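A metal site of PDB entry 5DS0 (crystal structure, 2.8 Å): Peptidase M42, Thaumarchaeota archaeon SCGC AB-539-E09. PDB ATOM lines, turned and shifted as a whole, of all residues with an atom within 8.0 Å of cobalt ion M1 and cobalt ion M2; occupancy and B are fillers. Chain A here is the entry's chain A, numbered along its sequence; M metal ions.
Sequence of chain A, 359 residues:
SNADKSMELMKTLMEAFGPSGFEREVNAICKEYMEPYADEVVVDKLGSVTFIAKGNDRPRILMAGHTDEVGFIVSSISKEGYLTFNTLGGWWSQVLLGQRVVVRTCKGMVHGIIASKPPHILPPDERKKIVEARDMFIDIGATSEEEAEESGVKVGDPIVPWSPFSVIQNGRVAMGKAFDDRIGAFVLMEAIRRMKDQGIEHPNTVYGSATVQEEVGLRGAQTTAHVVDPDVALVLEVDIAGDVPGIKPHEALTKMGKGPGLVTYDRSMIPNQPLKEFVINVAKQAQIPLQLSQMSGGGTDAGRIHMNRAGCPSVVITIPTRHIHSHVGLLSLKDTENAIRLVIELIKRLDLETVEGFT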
ATOM      1  N   GLY A  65      24.838   5.579  -3.636  1.00  0.00           N
ATOM      2  CA  GLY A  65      24.658   4.901  -4.928  1.00  0.00           C
ATOM      3  C   GLY A  65      23.454   5.504  -5.626  1.00  0.00           C
ATOM      4  O   GLY A  65      22.387   5.573  -5.047  1.00  0.00           O
ATOM      5  N   HIS A  66      23.620   5.944  -6.859  1.00  0.00           N
ATOM      6  CA  HIS A  66      22.513   6.631  -7.536  1.00  0.00           C
ATOM      7  C   HIS A  66      21.465   5.652  -8.077  1.00  0.00           C
ATOM      8  O   HIS A  66      21.819   4.614  -8.654  1.00  0.00           O
ATOM      9  CB  HIS A  66      23.018   7.587  -8.625  1.00  0.00           C
ATOM     10  CG  HIS A  66      23.651   6.915  -9.812  1.00  0.00           C
ATOM     11  ND1 HIS A  66      22.923   6.524 -10.915  1.00  0.00           N
ATOM     12  CD2 HIS A  66      24.940   6.607 -10.087  1.00  0.00           C
ATOM     13  CE1 HIS A  66      23.736   5.989 -11.814  1.00  0.00           C
ATOM     14  NE2 HIS A  66      24.974   6.034 -11.336  1.00  0.00           N
ATOM     15  N   THR A  67      20.203   5.978  -7.882  1.00  0.00           N
ATOM     16  CA  THR A  67      19.126   5.139  -8.327  1.00  0.00           C
ATOM     17  C   THR A  67      18.527   5.556  -9.667  1.00  0.00           C
ATOM     18  O   THR A  67      17.666   4.851 -10.210  1.00  0.00           O
ATOM     19  CB  THR A  67      17.973   5.143  -7.331  1.00  0.00           C
ATOM     20  OG1 THR A  67      17.592   6.494  -7.068  1.00  0.00           O
ATOM     21  CG2 THR A  67      18.402   4.457  -6.045  1.00  0.00           C
ATOM     22  N   ASP A  68      18.948   6.698 -10.199  1.00  0.00           N
ATOM     23  CA  ASP A  68      18.531   7.047 -11.546  1.00  0.00           C
ATOM     24  C   ASP A  68      19.256   6.156 -12.551  1.00  0.00           C
ATOM     25  O   ASP A  68      20.387   5.723 -12.315  1.00  0.00           O
ATOM     26  CB  ASP A  68      18.713   8.544 -11.859  1.00  0.00           C
ATOM     27  CG  ASP A  68      20.162   8.987 -11.897  1.00  0.00           C
ATOM     28  OD1 ASP A  68      20.933   8.609 -10.990  1.00  0.00           O
ATOM     29  OD2 ASP A  68      20.526   9.731 -12.829  1.00  0.00           O
ATOM     30  N   GLU A  69      18.565   5.865 -13.650  1.00  0.00           N
ATOM     31  CA  GLU A  69      19.127   5.085 -14.763  1.00  0.00           C
ATOM     32  C   GLU A  69      19.081   5.923 -16.016  1.00  0.00           C
ATOM     33  O   GLU A  69      18.293   6.859 -16.158  1.00  0.00           O
ATOM     34  CB  GLU A  69      18.313   3.813 -15.000  1.00  0.00           C
ATOM     35  CG  GLU A  69      16.838   4.094 -15.294  1.00  0.00           C
ATOM     36  CD  GLU A  69      16.019   2.852 -15.538  1.00  0.00           C
ATOM     37  OE1 GLU A  69      16.423   2.031 -16.395  1.00  0.00           O
ATOM     38  OE2 GLU A  69      14.946   2.713 -14.880  1.00  0.00           O
ATOM     39  N   VAL A  70      19.943   5.591 -16.945  1.00  0.00           N
ATOM     40  CA  VAL A  70      19.868   6.269 -18.232  1.00  0.00           C
ATOM     41  C   VAL A  70      18.526   5.959 -18.834  1.00  0.00           C
ATOM     42  O   VAL A  70      17.985   4.880 -18.632  1.00  0.00           O
ATOM     43  CB  VAL A  70      21.016   5.885 -19.174  1.00  0.00           C
ATOM     44  CG1 VAL A  70      22.343   6.361 -18.576  1.00  0.00           C
ATOM     45  CG2 VAL A  70      21.039   4.388 -19.433  1.00  0.00           C
ATOM     46  N   GLY A  89      20.985  11.165 -19.888  1.00  0.00           N
ATOM     47  CA  GLY A  89      22.237  10.488 -19.561  1.00  0.00           C
ATOM     48  C   GLY A  89      22.911  10.066 -20.850  1.00  0.00           C
ATOM     49  O   GLY A  89      22.329  10.189 -21.930  1.00  0.00           O
ATOM     50  N   GLY A  90      24.135   9.590 -20.739  1.00  0.00           N
ATOM     51  CA  GLY A  90      24.959   9.270 -21.904  1.00  0.00           C
ATOM     52  C   GLY A  90      24.611   7.922 -22.491  1.00  0.00           C
ATOM     53  O   GLY A  90      24.702   6.912 -21.803  1.00  0.00           O
ATOM     54  N   PHE A 179      21.750  -1.616 -13.535  1.00  0.00           N
ATOM     55  CA  PHE A 179      22.758  -1.962 -12.529  1.00  0.00           C
ATOM     56  C   PHE A 179      23.502  -0.711 -12.114  1.00  0.00           C
ATOM     57  O   PHE A 179      23.785  -0.525 -10.952  1.00  0.00           O
ATOM     58  CB  PHE A 179      23.736  -2.993 -13.060  1.00  0.00           C
ATOM     59  CG  PHE A 179      23.158  -4.368 -13.200  1.00  0.00           C
ATOM     60  CD1 PHE A 179      22.414  -4.935 -12.188  1.00  0.00           C
ATOM     61  CD2 PHE A 179      23.367  -5.100 -14.363  1.00  0.00           C
ATOM     62  CE1 PHE A 179      21.874  -6.193 -12.338  1.00  0.00           C
ATOM     63  CE2 PHE A 179      22.825  -6.377 -14.508  1.00  0.00           C
ATOM     64  CZ  PHE A 179      22.085  -6.914 -13.494  1.00  0.00           C
ATOM     65  N   ASP A 180      23.771   0.161 -13.083  1.00  0.00           N
ATOM     66  CA  ASP A 180      24.328   1.473 -12.824  1.00  0.00           C
ATOM     67  C   ASP A 180      23.155   2.395 -12.472  1.00  0.00           C
ATOM     68  O   ASP A 180      22.456   2.830 -13.360  1.00  0.00           O
ATOM     69  CB  ASP A 180      25.030   1.967 -14.082  1.00  0.00           C
ATOM     70  CG  ASP A 180      25.628   3.348 -13.946  1.00  0.00           C
ATOM     71  OD1 ASP A 180      25.749   3.863 -12.806  1.00  0.00           O
ATOM     72  OD2 ASP A 180      25.994   3.919 -14.994  1.00  0.00           O
ATOM     73  N   ASP A 181      22.931   2.721 -11.196  1.00  0.00           N
ATOM     74  CA  ASP A 181      23.777   2.306 -10.052  1.00  0.00           C
ATOM     75  C   ASP A 181      22.909   1.786  -8.913  1.00  0.00           C
ATOM     76  O   ASP A 181      23.161   2.021  -7.737  1.00  0.00           O
ATOM     77  CB  ASP A 181      24.638   3.491  -9.585  1.00  0.00           C
ATOM     78  CG  ASP A 181      25.646   3.109  -8.510  1.00  0.00           C
ATOM     79  OD1 ASP A 181      26.005   1.917  -8.382  1.00  0.00           O
ATOM     80  OD2 ASP A 181      26.109   4.046  -7.836  1.00  0.00           O
ATOM     81  N   ARG A 182      21.881   1.029  -9.290  1.00  0.00           N
ATOM     82  CA  ARG A 182      21.000   0.452  -8.311  1.00  0.00           C
ATOM     83  C   ARG A 182      21.703  -0.696  -7.585  1.00  0.00           C
ATOM     84  O   ARG A 182      21.343  -1.018  -6.448  1.00  0.00           O
ATOM     85  CB  ARG A 182      19.685   0.015  -8.950  1.00  0.00           C
ATOM     86  CG  ARG A 182      18.814   1.223  -9.267  1.00  0.00           C
ATOM     87  CD  ARG A 182      17.571   0.895 -10.104  1.00  0.00           C
ATOM     88  NE  ARG A 182      17.066   2.104 -10.765  1.00  0.00           N
ATOM     89  CZ  ARG A 182      16.106   2.124 -11.673  1.00  0.00           C
ATOM     90  NH1 ARG A 182      15.498   0.993 -12.028  1.00  0.00           N
ATOM     91  NH2 ARG A 182      15.724   3.271 -12.221  1.00  0.00           N
ATOM     92  N   GLU A 214      22.364  11.426 -11.047  1.00  0.00           N
ATOM     93  CA  GLU A 214      23.804  11.281 -11.294  1.00  0.00           C
ATOM     94  C   GLU A 214      24.091  11.343 -12.777  1.00  0.00           C
ATOM     95  O   GLU A 214      25.043  11.993 -13.193  1.00  0.00           O
ATOM     96  CB  GLU A 214      24.348   9.944 -10.755  1.00  0.00           C
ATOM     97  CG  GLU A 214      25.893   9.790 -10.714  1.00  0.00           C
ATOM     98  CD  GLU A 214      26.557   9.237 -11.993  1.00  0.00           C
ATOM     99  OE1 GLU A 214      25.956   8.448 -12.776  1.00  0.00           O
ATOM    100  OE2 GLU A 214      27.741   9.579 -12.214  1.00  0.00           O
ATOM    101  N   GLU A 215      23.271  10.646 -13.564  1.00  0.00           N
ATOM    102  CA  GLU A 215      23.590  10.420 -14.977  1.00  0.00           C
ATOM    103  C   GLU A 215      23.510  11.706 -15.809  1.00  0.00           C
ATOM    104  O   GLU A 215      23.984  11.724 -16.934  1.00  0.00           O
ATOM    105  CB  GLU A 215      22.720   9.317 -15.585  1.00  0.00           C
ATOM    106  CG  GLU A 215      22.831   7.935 -14.920  1.00  0.00           C
ATOM    107  CD  GLU A 215      24.068   7.102 -15.299  1.00  0.00           C
ATOM    108  OE1 GLU A 215      24.021   5.846 -15.283  1.00  0.00           O
ATOM    109  OE2 GLU A 215      25.101   7.693 -15.609  1.00  0.00           O
ATOM    110  N   VAL A 216      22.946  12.770 -15.244  1.00  0.00           N
ATOM    111  CA  VAL A 216      22.828  14.062 -15.939  1.00  0.00           C
ATOM    112  C   VAL A 216      23.682  15.190 -15.324  1.00  0.00           C
ATOM    113  O   VAL A 216      23.525  16.331 -15.723  1.00  0.00           O
ATOM    114  CB  VAL A 216      21.354  14.564 -16.045  1.00  0.00           C
ATOM    115  CG1 VAL A 216      20.508  13.602 -16.874  1.00  0.00           C
ATOM    116  CG2 VAL A 216      20.716  14.783 -14.675  1.00  0.00           C
ATOM    117  N   LEU A 218      25.658  14.719 -11.717  1.00  0.00           N
ATOM    118  CA  LEU A 218      25.966  14.537 -10.301  1.00  0.00           C
ATOM    119  C   LEU A 218      25.148  15.479  -9.399  1.00  0.00           C
ATOM    120  O   LEU A 218      25.631  15.976  -8.382  1.00  0.00           O
ATOM    121  CB  LEU A 218      27.470  14.727 -10.063  1.00  0.00           C
ATOM    122  CG  LEU A 218      28.390  14.135 -11.138  1.00  0.00           C
ATOM    123  CD1 LEU A 218      29.855  14.498 -10.851  1.00  0.00           C
ATOM    124  CD2 LEU A 218      28.200  12.629 -11.255  1.00  0.00           C
ATOM    125  N   VAL A 235      31.649   6.031  -2.125  1.00  0.00           N
ATOM    126  CA  VAL A 235      30.719   6.024  -3.216  1.00  0.00           C
ATOM    127  C   VAL A 235      30.751   4.677  -3.881  1.00  0.00           C
ATOM    128  O   VAL A 235      31.820   4.170  -4.209  1.00  0.00           O
ATOM    129  CB  VAL A 235      31.045   7.140  -4.216  1.00  0.00           C
ATOM    130  CG1 VAL A 235      30.200   6.989  -5.471  1.00  0.00           C
ATOM    131  CG2 VAL A 235      30.787   8.483  -3.564  1.00  0.00           C
ATOM    132  N   LEU A 236      29.574   4.105  -4.095  1.00  0.00           N
ATOM    133  CA  LEU A 236      29.444   2.817  -4.742  1.00  0.00           C
ATOM    134  C   LEU A 236      28.937   3.019  -6.148  1.00  0.00           C
ATOM    135  O   LEU A 236      27.935   3.669  -6.356  1.00  0.00           O
ATOM    136  CB  LEU A 236      28.476   1.942  -3.975  1.00  0.00           C
ATOM    137  CG  LEU A 236      29.007   1.705  -2.574  1.00  0.00           C
ATOM    138  CD1 LEU A 236      27.923   1.425  -1.554  1.00  0.00           C
ATOM    139  CD2 LEU A 236      29.991   0.564  -2.607  1.00  0.00           C
ATOM    140  N   GLU A 237      29.658   2.459  -7.113  1.00  0.00           N
ATOM    141  CA  GLU A 237      29.339   2.626  -8.514  1.00  0.00           C
ATOM    142  C   GLU A 237      29.607   1.318  -9.226  1.00  0.00           C
ATOM    143  O   GLU A 237      29.999   0.329  -8.622  1.00  0.00           O
ATOM    144  CB  GLU A 237      30.204   3.735  -9.144  1.00  0.00           C
ATOM    145  CG  GLU A 237      29.522   5.076  -9.400  1.00  0.00           C
ATOM    146  CD  GLU A 237      28.416   5.092 -10.454  1.00  0.00           C
ATOM    147  OE1 GLU A 237      28.087   4.074 -11.086  1.00  0.00           O
ATOM    148  OE2 GLU A 237      27.842   6.184 -10.647  1.00  0.00           O
ATOM    149  N   VAL A 238      29.362   1.322 -10.528  1.00  0.00           N
ATOM    150  CA  VAL A 238      29.754   0.232 -11.386  1.00  0.00           C
ATOM    151  C   VAL A 238      31.068   0.608 -12.043  1.00  0.00           C
ATOM    152  O   VAL A 238      31.421   1.776 -12.119  1.00  0.00           O
ATOM    153  CB  VAL A 238      28.698  -0.072 -12.448  1.00  0.00           C
ATOM    154  CG1 VAL A 238      27.432  -0.591 -11.796  1.00  0.00           C
ATOM    155  CG2 VAL A 238      28.397   1.170 -13.285  1.00  0.00           C
ATOM    156  N   ASP A 239      31.792  -0.392 -12.508  1.00  0.00           N
ATOM    157  CA  ASP A 239      32.989  -0.190 -13.267  1.00  0.00           C
ATOM    158  C   ASP A 239      32.731  -0.811 -14.624  1.00  0.00           C
ATOM    159  O   ASP A 239      32.077  -1.862 -14.714  1.00  0.00           O
ATOM    160  CB  ASP A 239      34.175  -0.898 -12.585  1.00  0.00           C
ATOM    161  CG  ASP A 239      35.453  -0.048 -12.538  1.00  0.00           C
ATOM    162  OD1 ASP A 239      35.754   0.658 -13.536  1.00  0.00           O
ATOM    163  OD2 ASP A 239      36.148  -0.091 -11.489  1.00  0.00           O
ATOM    164  N   ILE A 240      33.228  -0.186 -15.670  1.00  0.00           N
ATOM    165  CA  ILE A 240      33.148  -0.799 -16.979  1.00  0.00           C
ATOM    166  C   ILE A 240      34.095  -1.998 -16.973  1.00  0.00           C
ATOM    167  O   ILE A 240      35.279  -1.845 -16.729  1.00  0.00           O
ATOM    168  CB  ILE A 240      33.549   0.162 -18.108  1.00  0.00           C
ATOM    169  CG1 ILE A 240      32.583   1.353 -18.202  1.00  0.00           C
ATOM    170  CG2 ILE A 240      33.579  -0.576 -19.443  1.00  0.00           C
ATOM    171  CD1 ILE A 240      33.133   2.659 -17.672  1.00  0.00           C
ATOM    172  N   GLY A 299      32.923  10.045 -14.499  1.00  0.00           N
ATOM    173  CA  GLY A 299      32.854  10.595 -13.147  1.00  0.00           C
ATOM    174  C   GLY A 299      31.820   9.897 -12.288  1.00  0.00           C
ATOM    175  O   GLY A 299      31.118   9.001 -12.756  1.00  0.00           O
ATOM    176  N   THR A 300      31.745  10.324 -11.022  1.00  0.00           N
ATOM    177  CA  THR A 300      30.909   9.689  -9.995  1.00  0.00           C
ATOM    178  C   THR A 300      30.302  10.724  -9.057  1.00  0.00           C
ATOM    179  O   THR A 300      30.731  11.879  -9.056  1.00  0.00           O
ATOM    180  CB  THR A 300      31.726   8.727  -9.118  1.00  0.00           C
ATOM    181  OG1 THR A 300      32.852   9.429  -8.566  1.00  0.00           O
ATOM    182  CG2 THR A 300      32.221   7.569  -9.943  1.00  0.00           C
ATOM    183  N   ASP A 301      29.319  10.313  -8.268  1.00  0.00           N
ATOM    184  CA  ASP A 301      28.765  11.163  -7.202  1.00  0.00           C
ATOM    185  C   ASP A 301      29.910  11.765  -6.362  1.00  0.00           C
ATOM    186  O   ASP A 301      29.779  12.883  -5.841  1.00  0.00           O
ATOM    187  CB  ASP A 301      27.857  10.375  -6.256  1.00  0.00           C
ATOM    188  CG  ASP A 301      26.494  10.002  -6.873  1.00  0.00           C
ATOM    189  OD1 ASP A 301      25.884  10.838  -7.593  1.00  0.00           O
ATOM    190  OD2 ASP A 301      26.044   8.862  -6.565  1.00  0.00           O
ATOM    191  N   ILE A 324      27.124  -1.501 -19.387  1.00  0.00           N
ATOM    192  CA  ILE A 324      26.355  -0.446 -18.722  1.00  0.00           C
ATOM    193  C   ILE A 324      25.862   0.583 -19.736  1.00  0.00           C
ATOM    194  O   ILE A 324      26.264   0.550 -20.902  1.00  0.00           O
ATOM    195  CB  ILE A 324      27.163   0.271 -17.639  1.00  0.00           C
ATOM    196  CG1 ILE A 324      28.382   0.966 -18.231  1.00  0.00           C
ATOM    197  CG2 ILE A 324      27.585  -0.726 -16.572  1.00  0.00           C
ATOM    198  CD1 ILE A 324      29.003   1.995 -17.298  1.00  0.00           C
ATOM    199  N   HIS A 325      24.973   1.463 -19.307  1.00  0.00           N
ATOM    200  CA  HIS A 325      24.376   2.467 -20.189  1.00  0.00           C
ATOM    201  C   HIS A 325      23.826   1.823 -21.464  1.00  0.00           C
ATOM    202  O   HIS A 325      23.968   2.359 -22.570  1.00  0.00           O
ATOM    203  CB  HIS A 325      25.396   3.562 -20.526  1.00  0.00           C
ATOM    204  CG  HIS A 325      25.702   4.477 -19.384  1.00  0.00           C
ATOM    205  ND1 HIS A 325      25.942   5.821 -19.567  1.00  0.00           N
ATOM    206  CD2 HIS A 325      25.792   4.253 -18.056  1.00  0.00           C
ATOM    207  CE1 HIS A 325      26.174   6.382 -18.389  1.00  0.00           C
ATOM    208  NE2 HIS A 325      26.086   5.454 -17.461  1.00  0.00           N
HETATM  209 CO    CO M   1      26.286   5.696 -15.373  1.00  0.00          CO
HETATM  210 CO    CO M   2      26.640   5.623 -12.346  1.00  0.00          CO
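Cobalt ion M2 is bound by NE2 of His 66 (2.0 Å), OD1 of Asp 180 (2.0 Å), OE2 of Glu 237 (2.2 Å) and OE1 of Glu 237 (2.5 Å).
Cobalt ion M1 is bound by OD2 of Asp 180 (1.8 Å), NE2 of His 325 (2.1 Å), OE1 of Glu 215 (2.3 Å) and OE2 of Glu 215 (2.3 Å).
Merely in contact with cobalt ion M1: Glu 214.
Four residues have an atom within 4 Å of cobalt ion M1: Asp 180, Glu 214, Glu 215 and His 325.
OD2 of Asp 68 lies within hydrogen-bond range of N of Glu 214.
The backbone NH of Glu 215 sits at hydrogen-bond distance from the side-chain carboxylate of Asp 68, 3.0 Å away.
The side-chain carboxylate (OD1) of Asp 68 sits at hydrogen-bond distance from a ring nitrogen (ND1) of His 66.
The side-chain carboxylate (OE1) of Glu 214 lies close to a ring nitrogen (NE2) of His 66 (3.0 Å).
The backbone carbonyl oxygen of Gly 90 sits at hydrogen-bond distance from a ring nitrogen (ND1) of His 325, 2.8 Å away.
The backbone NH (N) of His 66 is in hydrogen-bond range of the side-chain carboxylate (OD2) of Asp 181 (3.3 Å).
OE1 of Glu 214 touches cobalt ion M2, at 2.9 Å.
Five residues have an atom within 4 Å of cobalt ion M2: His 66, Asp 180, Glu 214, Glu 215 and Glu 237.
Along chain A the residues within 4 Å of cobalt ion M2 span positions 66 to 237.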
